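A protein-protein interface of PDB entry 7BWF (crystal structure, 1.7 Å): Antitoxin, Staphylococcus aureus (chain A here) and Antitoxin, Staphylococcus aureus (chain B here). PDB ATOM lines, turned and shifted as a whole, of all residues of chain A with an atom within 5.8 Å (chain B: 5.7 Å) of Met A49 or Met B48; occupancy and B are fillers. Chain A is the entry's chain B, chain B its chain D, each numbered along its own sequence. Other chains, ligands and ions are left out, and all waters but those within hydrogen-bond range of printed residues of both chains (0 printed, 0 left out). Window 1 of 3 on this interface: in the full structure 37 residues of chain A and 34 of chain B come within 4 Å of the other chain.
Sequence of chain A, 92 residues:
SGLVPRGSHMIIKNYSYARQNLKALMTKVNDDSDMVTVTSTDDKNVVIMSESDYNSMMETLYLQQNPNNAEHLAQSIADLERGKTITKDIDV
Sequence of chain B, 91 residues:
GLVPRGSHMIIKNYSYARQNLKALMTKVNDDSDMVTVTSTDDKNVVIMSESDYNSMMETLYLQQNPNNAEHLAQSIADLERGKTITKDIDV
Printed residues of chain A that touch a printed residue of chain B: Val A29, Met A35, Asn A45, Val A46, Val A47, Ile A48, Met A49, Ser A50, Glu A51, Tyr A54 and Met A57.
Hydrophobic or aromatic side chains of chain A that line the printed part of chain B: Val A29, Met A35, Val A46, Val A47, Ile A48, Met A49, Tyr A54 and Met A57.
Among the printed residues, 25 pairs touch across the chains.
Among the printed residues, no Asp or Glu carboxylate lies within 4 Å of a Lys or Arg side-chain nitrogen of the other chain.
The backbone NH (N) of Ile A48 sits at hydrogen-bond distance from the backbone carbonyl oxygen (O) of Val A36 (2.7 Å).
The backbone NH of Tyr A54 lies close to the side-chain sulfur of Met A49.
The side-chain hydroxyl of Ser A50 is in hydrogen-bond range of the backbone NH of Asp A53 (3.0 Å).
N of Ile B47 is in hydrogen-bond range of O of Val B35, 2.7 Å away.
The side-chain sulfur (SD) of Met B48 lies close to the backbone NH (N) of Tyr B53 (3.6 Å).
The backbone NH (N) of Asp B52 is in hydrogen-bond range of the side-chain hydroxyl (OG) of Ser B49.
The side-chain hydroxyl (OH) of Tyr B53 lies close to the side-chain sulfur (SD) of Met A35 (3.8 Å).
OE1 of Glu B50 is in hydrogen-bond range of ND2 of Asn A45 (3.0 Å).
N of Val A47 is in hydrogen-bond range of O of Met B48, 2.8 Å away.
The backbone NH (N) of Val B46 lies within hydrogen-bond range of the backbone carbonyl oxygen (O) of Met A49 (2.7 Å).
The backbone NH (N) of Glu A51 lies within hydrogen-bond range of the backbone carbonyl oxygen (O) of Asn B44 (3.1 Å).
The side-chain hydroxyl of Tyr A54 lies close to the side-chain sulfur of Met B34 (3.8 Å).
Met A49 touches just these residues of chain B: Val B45 (3.1 Å), Val B46 (2.7 Å), Met B48 (3.8 Å) and Tyr B53 (3.6 Å).
Met B48 touches four residues of chain A.
Of the printed residues of chain B, Val A46 touches Val B28 (3.5 Å), Ile B47 (3.7 Å), Met B48 (3.1 Å) and Glu B50 (3.8 Å).
Of the printed residues of chain B, Glu A51 touches Asn B44 and Val B45.
Of the printed residues of chain B, Asn A45 touches Ser B49 and Glu B50.
Of the printed residues of chain A, Ser B49 touches Asn A45 (3.6 Å).
The nearest residue of chain A that does not touch Met B48 is Asn A45 (4.5 Å).
Asn A45 touches Ser B49.
CG1 of Val A46 touches CG2 of Val B28, 3.5 Å away.
Val A46 touches Ile B47 (CB to CG2, 3.7 Å).
Val A46 touches Glu B50.
CA of Ile B47 touches O of Val A47 (3.6 Å).
Tyr B53 touches Val A47.
Met A49 touches Val B45 (O to CA, 3.1 Å).
Met A49 touches Tyr B53 (CE to CD1, 3.6 Å).
Met B48 touches Tyr A54.
CE of Met A57 touches CE of Met B56 (3.1 Å).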
ATOM      1  N   VAL A  29      30.761 -34.486 -22.173  1.00  0.00           N
ATOM      2  CA  VAL A  29      31.172 -33.096 -22.356  1.00  0.00           C
ATOM      3  C   VAL A  29      31.604 -32.490 -21.029  1.00  0.00           C
ATOM      4  O   VAL A  29      32.429 -31.573 -20.999  1.00  0.00           O
ATOM      5  CB  VAL A  29      30.044 -32.277 -23.010  1.00  0.00           C
ATOM      6  CG1 VAL A  29      29.758 -32.826 -24.400  1.00  0.00           C
ATOM      7  CG2 VAL A  29      28.817 -32.287 -22.126  1.00  0.00           C
ATOM      8  N   ASP A  34      34.931 -31.929 -23.916  1.00  0.00           N
ATOM      9  CA  ASP A  34      34.591 -32.136 -25.314  1.00  0.00           C
ATOM     10  C   ASP A  34      33.223 -31.540 -25.625  1.00  0.00           C
ATOM     11  O   ASP A  34      32.448 -31.173 -24.738  1.00  0.00           O
ATOM     12  CB  ASP A  34      34.638 -33.629 -25.676  1.00  0.00           C
ATOM     13  CG  ASP A  34      36.073 -34.156 -25.771  1.00  0.00           C
ATOM     14  OD1 ASP A  34      37.000 -33.343 -25.934  1.00  0.00           O
ATOM     15  OD2 ASP A  34      36.281 -35.372 -25.666  1.00  0.00           O
ATOM     16  N   MET A  35      32.957 -31.415 -26.920  1.00  0.00           N
ATOM     17  CA  MET A  35      31.717 -30.865 -27.433  1.00  0.00           C
ATOM     18  C   MET A  35      31.190 -31.808 -28.497  1.00  0.00           C
ATOM     19  O   MET A  35      31.956 -32.500 -29.176  1.00  0.00           O
ATOM     20  CB  MET A  35      31.925 -29.458 -27.999  1.00  0.00           C
ATOM     21  CG  MET A  35      32.483 -28.517 -26.945  1.00  0.00           C
ATOM     22  SD  MET A  35      32.686 -26.809 -27.496  1.00  0.00           S
ATOM     23  CE  MET A  35      33.456 -26.090 -26.042  1.00  0.00           C
ATOM     24  N   VAL A  36      29.870 -31.836 -28.610  1.00  0.00           N
ATOM     25  CA  VAL A  36      29.172 -32.763 -29.481  1.00  0.00           C
ATOM     26  C   VAL A  36      28.305 -31.948 -30.426  1.00  0.00           C
ATOM     27  O   VAL A  36      27.406 -31.218 -29.985  1.00  0.00           O
ATOM     28  CB  VAL A  36      28.320 -33.765 -28.689  1.00  0.00           C
ATOM     29  CG1 VAL A  36      27.520 -34.625 -29.647  1.00  0.00           C
ATOM     30  CG2 VAL A  36      29.197 -34.600 -27.775  1.00  0.00           C
ATOM     31  N   ASN A  45      21.301 -28.504 -37.106  1.00  0.00           N
ATOM     32  CA  ASN A  45      22.108 -29.186 -36.108  1.00  0.00           C
ATOM     33  C   ASN A  45      22.300 -28.326 -34.860  1.00  0.00           C
ATOM     34  O   ASN A  45      22.021 -27.125 -34.844  1.00  0.00           O
ATOM     35  CB  ASN A  45      23.477 -29.558 -36.684  1.00  0.00           C
ATOM     36  CG  ASN A  45      23.388 -30.242 -38.039  1.00  0.00           C
ATOM     37  OD1 ASN A  45      22.401 -30.907 -38.362  1.00  0.00           O
ATOM     38  ND2 ASN A  45      24.427 -30.066 -38.849  1.00  0.00           N
ATOM     39  N   VAL A  46      22.809 -28.962 -33.808  1.00  0.00           N
ATOM     40  CA  VAL A  46      23.124 -28.272 -32.565  1.00  0.00           C
ATOM     41  C   VAL A  46      24.514 -28.678 -32.094  1.00  0.00           C
ATOM     42  O   VAL A  46      25.088 -29.681 -32.532  1.00  0.00           O
ATOM     43  CB  VAL A  46      22.093 -28.563 -31.448  1.00  0.00           C
ATOM     44  CG1 VAL A  46      20.723 -28.079 -31.856  1.00  0.00           C
ATOM     45  CG2 VAL A  46      22.083 -30.049 -31.119  1.00  0.00           C
ATOM     46  N   VAL A  47      25.044 -27.877 -31.170  1.00  0.00           N
ATOM     47  CA  VAL A  47      26.269 -28.194 -30.447  1.00  0.00           C
ATOM     48  C   VAL A  47      25.928 -28.301 -28.965  1.00  0.00           C
ATOM     49  O   VAL A  47      25.241 -27.429 -28.416  1.00  0.00           O
ATOM     50  CB  VAL A  47      27.363 -27.137 -30.681  1.00  0.00           C
ATOM     51  CG1 VAL A  47      28.535 -27.367 -29.728  1.00  0.00           C
ATOM     52  CG2 VAL A  47      27.814 -27.171 -32.133  1.00  0.00           C
ATOM     53  N   ILE A  48      26.398 -29.370 -28.325  1.00  0.00           N
ATOM     54  CA  ILE A  48      26.207 -29.590 -26.894  1.00  0.00           C
ATOM     55  C   ILE A  48      27.557 -29.418 -26.212  1.00  0.00           C
ATOM     56  O   ILE A  48      28.539 -30.078 -26.579  1.00  0.00           O
ATOM     57  CB  ILE A  48      25.623 -30.980 -26.594  1.00  0.00           C
ATOM     58  CG1 ILE A  48      24.350 -31.209 -27.411  1.00  0.00           C
ATOM     59  CG2 ILE A  48      25.307 -31.115 -25.118  1.00  0.00           C
ATOM     60  CD1 ILE A  48      23.669 -32.560 -27.173  1.00  0.00           C
ATOM     61  N   MET A  49      27.599 -28.537 -25.217  1.00  0.00           N
ATOM     62  CA  MET A  49      28.773 -28.307 -24.391  1.00  0.00           C
ATOM     63  C   MET A  49      28.346 -28.285 -22.930  1.00  0.00           C
ATOM     64  O   MET A  49      27.168 -28.110 -22.600  1.00  0.00           O
ATOM     65  CB  MET A  49      29.475 -26.987 -24.752  1.00  0.00           C
ATOM     66  CG  MET A  49      28.639 -25.741 -24.494  1.00  0.00           C
ATOM     67  SD  MET A  49      29.495 -24.225 -24.963  1.00  0.00           S
ATOM     68  CE  MET A  49      29.637 -24.450 -26.735  1.00  0.00           C
ATOM     69  N   SER A  50      29.320 -28.483 -22.050  1.00  0.00           N
ATOM     70  CA  SER A  50      29.055 -28.392 -20.624  1.00  0.00           C
ATOM     71  C   SER A  50      28.638 -26.967 -20.283  1.00  0.00           C
ATOM     72  O   SER A  50      29.067 -26.006 -20.923  1.00  0.00           O
ATOM     73  CB  SER A  50      30.293 -28.792 -19.812  1.00  0.00           C
ATOM     74  OG  SER A  50      31.339 -27.843 -19.928  1.00  0.00           O
ATOM     75  N   GLU A  51      27.759 -26.837 -19.288  1.00  0.00           N
ATOM     76  CA  GLU A  51      27.369 -25.511 -18.823  1.00  0.00           C
ATOM     77  C   GLU A  51      28.600 -24.708 -18.413  1.00  0.00           C
ATOM     78  O   GLU A  51      28.667 -23.494 -18.638  1.00  0.00           O
ATOM     79  CB  GLU A  51      26.387 -25.623 -17.649  1.00  0.00           C
ATOM     80  CG  GLU A  51      25.861 -24.277 -17.162  1.00  0.00           C
ATOM     81  CD  GLU A  51      24.836 -24.431 -16.044  1.00  0.00           C
ATOM     82  OE1 GLU A  51      24.908 -25.438 -15.312  1.00  0.00           O
ATOM     83  OE2 GLU A  51      23.971 -23.552 -15.893  1.00  0.00           O
ATOM     84  N   ASP A  53      31.795 -24.922 -19.598  1.00  0.00           N
ATOM     85  CA  ASP A  53      32.451 -24.407 -20.798  1.00  0.00           C
ATOM     86  C   ASP A  53      31.632 -23.298 -21.434  1.00  0.00           C
ATOM     87  O   ASP A  53      32.187 -22.314 -21.930  1.00  0.00           O
ATOM     88  CB  ASP A  53      32.692 -25.533 -21.799  1.00  0.00           C
ATOM     89  CG  ASP A  53      33.859 -26.410 -21.402  1.00  0.00           C
ATOM     90  OD1 ASP A  53      34.621 -26.010 -20.494  1.00  0.00           O
ATOM     91  OD2 ASP A  53      34.004 -27.504 -21.971  1.00  0.00           O
ATOM     92  N   TYR A  54      30.307 -23.411 -21.393  1.00  0.00           N
ATOM     93  CA  TYR A  54      29.490 -22.322 -21.904  1.00  0.00           C
ATOM     94  C   TYR A  54      29.772 -21.035 -21.143  1.00  0.00           C
ATOM     95  O   TYR A  54      30.042 -19.991 -21.742  1.00  0.00           O
ATOM     96  CB  TYR A  54      28.011 -22.643 -21.791  1.00  0.00           C
ATOM     97  CG  TYR A  54      27.170 -21.442 -22.154  1.00  0.00           C
ATOM     98  CD1 TYR A  54      27.146 -20.971 -23.451  1.00  0.00           C
ATOM     99  CD2 TYR A  54      26.451 -20.744 -21.192  1.00  0.00           C
ATOM    100  CE1 TYR A  54      26.400 -19.875 -23.800  1.00  0.00           C
ATOM    101  CE2 TYR A  54      25.683 -19.635 -21.536  1.00  0.00           C
ATOM    102  CZ  TYR A  54      25.656 -19.215 -22.854  1.00  0.00           C
ATOM    103  OH  TYR A  54      24.922 -18.119 -23.262  1.00  0.00           O
ATOM    104  N   MET A  57      33.124 -19.563 -22.002  1.00  0.00           N
ATOM    105  CA  MET A  57      33.170 -18.879 -23.292  1.00  0.00           C
ATOM    106  C   MET A  57      32.553 -17.485 -23.200  1.00  0.00           C
ATOM    107  O   MET A  57      33.125 -16.514 -23.700  1.00  0.00           O
ATOM    108  CB  MET A  57      32.454 -19.711 -24.365  1.00  0.00           C
ATOM    109  CG  MET A  57      33.113 -21.044 -24.665  1.00  0.00           C
ATOM    110  SD  MET A  57      32.280 -21.980 -25.966  1.00  0.00           S
ATOM    111  CE  MET A  57      31.595 -20.693 -27.016  1.00  0.00           C
ATOM    112  N   VAL B  28      16.151 -24.068 -30.905  1.00  0.00           N
ATOM    113  CA  VAL B  28      17.364 -23.258 -30.815  1.00  0.00           C
ATOM    114  C   VAL B  28      17.802 -22.804 -32.201  1.00  0.00           C
ATOM    115  O   VAL B  28      18.421 -21.748 -32.346  1.00  0.00           O
ATOM    116  CB  VAL B  28      18.489 -24.027 -30.092  1.00  0.00           C
ATOM    117  CG1 VAL B  28      18.016 -24.459 -28.711  1.00  0.00           C
ATOM    118  CG2 VAL B  28      18.937 -25.207 -30.933  1.00  0.00           C
ATOM    119  N   ASP B  33      17.477 -19.296 -29.596  1.00  0.00           N
ATOM    120  CA  ASP B  33      17.493 -19.513 -28.159  1.00  0.00           C
ATOM    121  C   ASP B  33      18.470 -20.632 -27.819  1.00  0.00           C
ATOM    122  O   ASP B  33      19.026 -21.301 -28.693  1.00  0.00           O
ATOM    123  CB  ASP B  33      16.088 -19.840 -27.645  1.00  0.00           C
ATOM    124  CG  ASP B  33      15.175 -18.608 -27.616  1.00  0.00           C
ATOM    125  OD1 ASP B  33      15.682 -17.483 -27.768  1.00  0.00           O
ATOM    126  OD2 ASP B  33      13.948 -18.764 -27.488  1.00  0.00           O
ATOM    127  N   MET B  34      18.709 -20.794 -26.524  1.00  0.00           N
ATOM    128  CA  MET B  34      19.634 -21.785 -26.006  1.00  0.00           C
ATOM    129  C   MET B  34      18.988 -22.444 -24.803  1.00  0.00           C
ATOM    130  O   MET B  34      18.201 -21.823 -24.080  1.00  0.00           O
ATOM    131  CB  MET B  34      20.981 -21.155 -25.630  1.00  0.00           C
ATOM    132  CG  MET B  34      21.555 -20.269 -26.723  1.00  0.00           C
ATOM    133  SD  MET B  34      22.497 -18.882 -26.039  1.00  0.00           S
ATOM    134  CE  MET B  34      24.161 -19.526 -26.138  1.00  0.00           C
ATOM    135  N   VAL B  35      19.308 -23.717 -24.619  1.00  0.00           N
ATOM    136  CA  VAL B  35      18.670 -24.553 -23.617  1.00  0.00           C
ATOM    137  C   VAL B  35      19.754 -25.103 -22.708  1.00  0.00           C
ATOM    138  O   VAL B  35      20.700 -25.749 -23.174  1.00  0.00           O
ATOM    139  CB  VAL B  35      17.858 -25.695 -24.253  1.00  0.00           C
ATOM    140  CG1 VAL B  35      17.239 -26.560 -23.166  1.00  0.00           C
ATOM    141  CG2 VAL B  35      16.806 -25.126 -25.192  1.00  0.00           C
ATOM    142  N   ASN B  44      25.442 -30.368 -15.935  1.00  0.00           N
ATOM    143  CA  ASN B  44      24.515 -29.826 -16.916  1.00  0.00           C
ATOM    144  C   ASN B  44      25.215 -29.507 -18.236  1.00  0.00           C
ATOM    145  O   ASN B  44      26.443 -29.435 -18.327  1.00  0.00           O
ATOM    146  CB  ASN B  44      23.843 -28.563 -16.377  1.00  0.00           C
ATOM    147  CG  ASN B  44      23.223 -28.759 -15.004  1.00  0.00           C
ATOM    148  OD1 ASN B  44      22.929 -29.880 -14.582  1.00  0.00           O
ATOM    149  ND2 ASN B  44      23.031 -27.655 -14.291  1.00  0.00           N
ATOM    150  N   VAL B  45      24.398 -29.288 -19.267  1.00  0.00           N
ATOM    151  CA  VAL B  45      24.891 -28.928 -20.589  1.00  0.00           C
ATOM    152  C   VAL B  45      24.096 -27.740 -21.117  1.00  0.00           C
ATOM    153  O   VAL B  45      22.992 -27.433 -20.657  1.00  0.00           O
ATOM    154  CB  VAL B  45      24.813 -30.108 -21.589  1.00  0.00           C
ATOM    155  CG1 VAL B  45      25.578 -31.298 -21.050  1.00  0.00           C
ATOM    156  CG2 VAL B  45      23.357 -30.472 -21.893  1.00  0.00           C
ATOM    157  N   VAL B  46      24.685 -27.066 -22.102  1.00  0.00           N
ATOM    158  CA  VAL B  46      24.008 -26.026 -22.864  1.00  0.00           C
ATOM    159  C   VAL B  46      23.914 -26.487 -24.311  1.00  0.00           C
ATOM    160  O   VAL B  46      24.910 -26.937 -24.895  1.00  0.00           O
ATOM    161  CB  VAL B  46      24.738 -24.674 -22.774  1.00  0.00           C
ATOM    162  CG1 VAL B  46      24.238 -23.727 -23.860  1.00  0.00           C
ATOM    163  CG2 VAL B  46      24.560 -24.075 -21.386  1.00  0.00           C
ATOM    164  N   ILE B  47      22.718 -26.374 -24.887  1.00  0.00           N
ATOM    165  CA  ILE B  47      22.465 -26.724 -26.280  1.00  0.00           C
ATOM    166  C   ILE B  47      22.219 -25.440 -27.055  1.00  0.00           C
ATOM    167  O   ILE B  47      21.354 -24.635 -26.685  1.00  0.00           O
ATOM    168  CB  ILE B  47      21.266 -27.676 -26.429  1.00  0.00           C
ATOM    169  CG1 ILE B  47      21.457 -28.915 -25.553  1.00  0.00           C
ATOM    170  CG2 ILE B  47      21.101 -28.090 -27.876  1.00  0.00           C
ATOM    171  CD1 ILE B  47      20.290 -29.898 -25.575  1.00  0.00           C
ATOM    172  N   MET B  48      22.973 -25.257 -28.135  1.00  0.00           N
ATOM    173  CA  MET B  48      22.808 -24.134 -29.043  1.00  0.00           C
ATOM    174  C   MET B  48      22.847 -24.643 -30.475  1.00  0.00           C
ATOM    175  O   MET B  48      23.327 -25.746 -30.759  1.00  0.00           O
ATOM    176  CB  MET B  48      23.900 -23.070 -28.836  1.00  0.00           C
ATOM    177  CG  MET B  48      25.322 -23.563 -29.085  1.00  0.00           C
ATOM    178  SD  MET B  48      26.558 -22.267 -28.852  1.00  0.00           S
ATOM    179  CE  MET B  48      26.635 -22.198 -27.066  1.00  0.00           C
ATOM    180  N   SER B  49      22.309 -23.829 -31.375  1.00  0.00           N
ATOM    181  CA  SER B  49      22.396 -24.137 -32.793  1.00  0.00           C
ATOM    182  C   SER B  49      23.858 -24.155 -33.215  1.00  0.00           C
ATOM    183  O   SER B  49      24.692 -23.426 -32.673  1.00  0.00           O
ATOM    184  CB  SER B  49      21.614 -23.109 -33.619  1.00  0.00           C
ATOM    185  OG  SER B  49      22.311 -21.879 -33.732  1.00  0.00           O
ATOM    186  N   GLU B  50      24.176 -25.036 -34.164  1.00  0.00           N
ATOM    187  CA  GLU B  50      25.529 -25.079 -34.706  1.00  0.00           C
ATOM    188  C   GLU B  50      25.926 -23.710 -35.247  1.00  0.00           C
ATOM    189  O   GLU B  50      27.083 -23.294 -35.122  1.00  0.00           O
ATOM    190  CB  GLU B  50      25.627 -26.144 -35.803  1.00  0.00           C
ATOM    191  CG  GLU B  50      27.016 -26.257 -36.414  1.00  0.00           C
ATOM    192  CD  GLU B  50      27.110 -27.391 -37.429  1.00  0.00           C
ATOM    193  OE1 GLU B  50      26.074 -27.751 -38.021  1.00  0.00           O
ATOM    194  OE2 GLU B  50      28.219 -27.908 -37.640  1.00  0.00           O
ATOM    195  N   ASP B  52      24.936 -20.683 -34.162  1.00  0.00           N
ATOM    196  CA  ASP B  52      25.282 -19.796 -33.052  1.00  0.00           C
ATOM    197  C   ASP B  52      26.614 -20.186 -32.427  1.00  0.00           C
ATOM    198  O   ASP B  52      27.393 -19.318 -32.023  1.00  0.00           O
ATOM    199  CB  ASP B  52      24.170 -19.807 -32.003  1.00  0.00           C
ATOM    200  CG  ASP B  52      22.977 -18.958 -32.416  1.00  0.00           C
ATOM    201  OD1 ASP B  52      23.103 -18.162 -33.373  1.00  0.00           O
ATOM    202  OD2 ASP B  52      21.906 -19.097 -31.804  1.00  0.00           O
ATOM    203  N   TYR B  53      26.912 -21.484 -32.363  1.00  0.00           N
ATOM    204  CA  TYR B  53      28.229 -21.898 -31.895  1.00  0.00           C
ATOM    205  C   TYR B  53      29.313 -21.354 -32.814  1.00  0.00           C
ATOM    206  O   TYR B  53      30.282 -20.743 -32.356  1.00  0.00           O
ATOM    207  CB  TYR B  53      28.328 -23.419 -31.817  1.00  0.00           C
ATOM    208  CG  TYR B  53      29.744 -23.896 -31.542  1.00  0.00           C
ATOM    209  CD1 TYR B  53      30.248 -23.915 -30.248  1.00  0.00           C
ATOM    210  CD2 TYR B  53      30.576 -24.314 -32.572  1.00  0.00           C
ATOM    211  CE1 TYR B  53      31.537 -24.348 -29.987  1.00  0.00           C
ATOM    212  CE2 TYR B  53      31.869 -24.748 -32.319  1.00  0.00           C
ATOM    213  CZ  TYR B  53      32.344 -24.765 -31.022  1.00  0.00           C
ATOM    214  OH  TYR B  53      33.628 -25.193 -30.747  1.00  0.00           O
ATOM    215  N   MET B  56      29.810 -17.668 -32.314  1.00  0.00           N
ATOM    216  CA  MET B  56      30.516 -17.318 -31.084  1.00  0.00           C
ATOM    217  C   MET B  56      32.017 -17.539 -31.230  1.00  0.00           C
ATOM    218  O   MET B  56      32.823 -16.691 -30.833  1.00  0.00           O
ATOM    219  CB  MET B  56      29.953 -18.130 -29.913  1.00  0.00           C
ATOM    220  CG  MET B  56      28.965 -17.323 -29.092  1.00  0.00           C
ATOM    221  SD  MET B  56      27.720 -18.250 -28.206  1.00  0.00           S
ATOM    222  CE  MET B  56      28.737 -19.464 -27.404  1.00  0.00           C
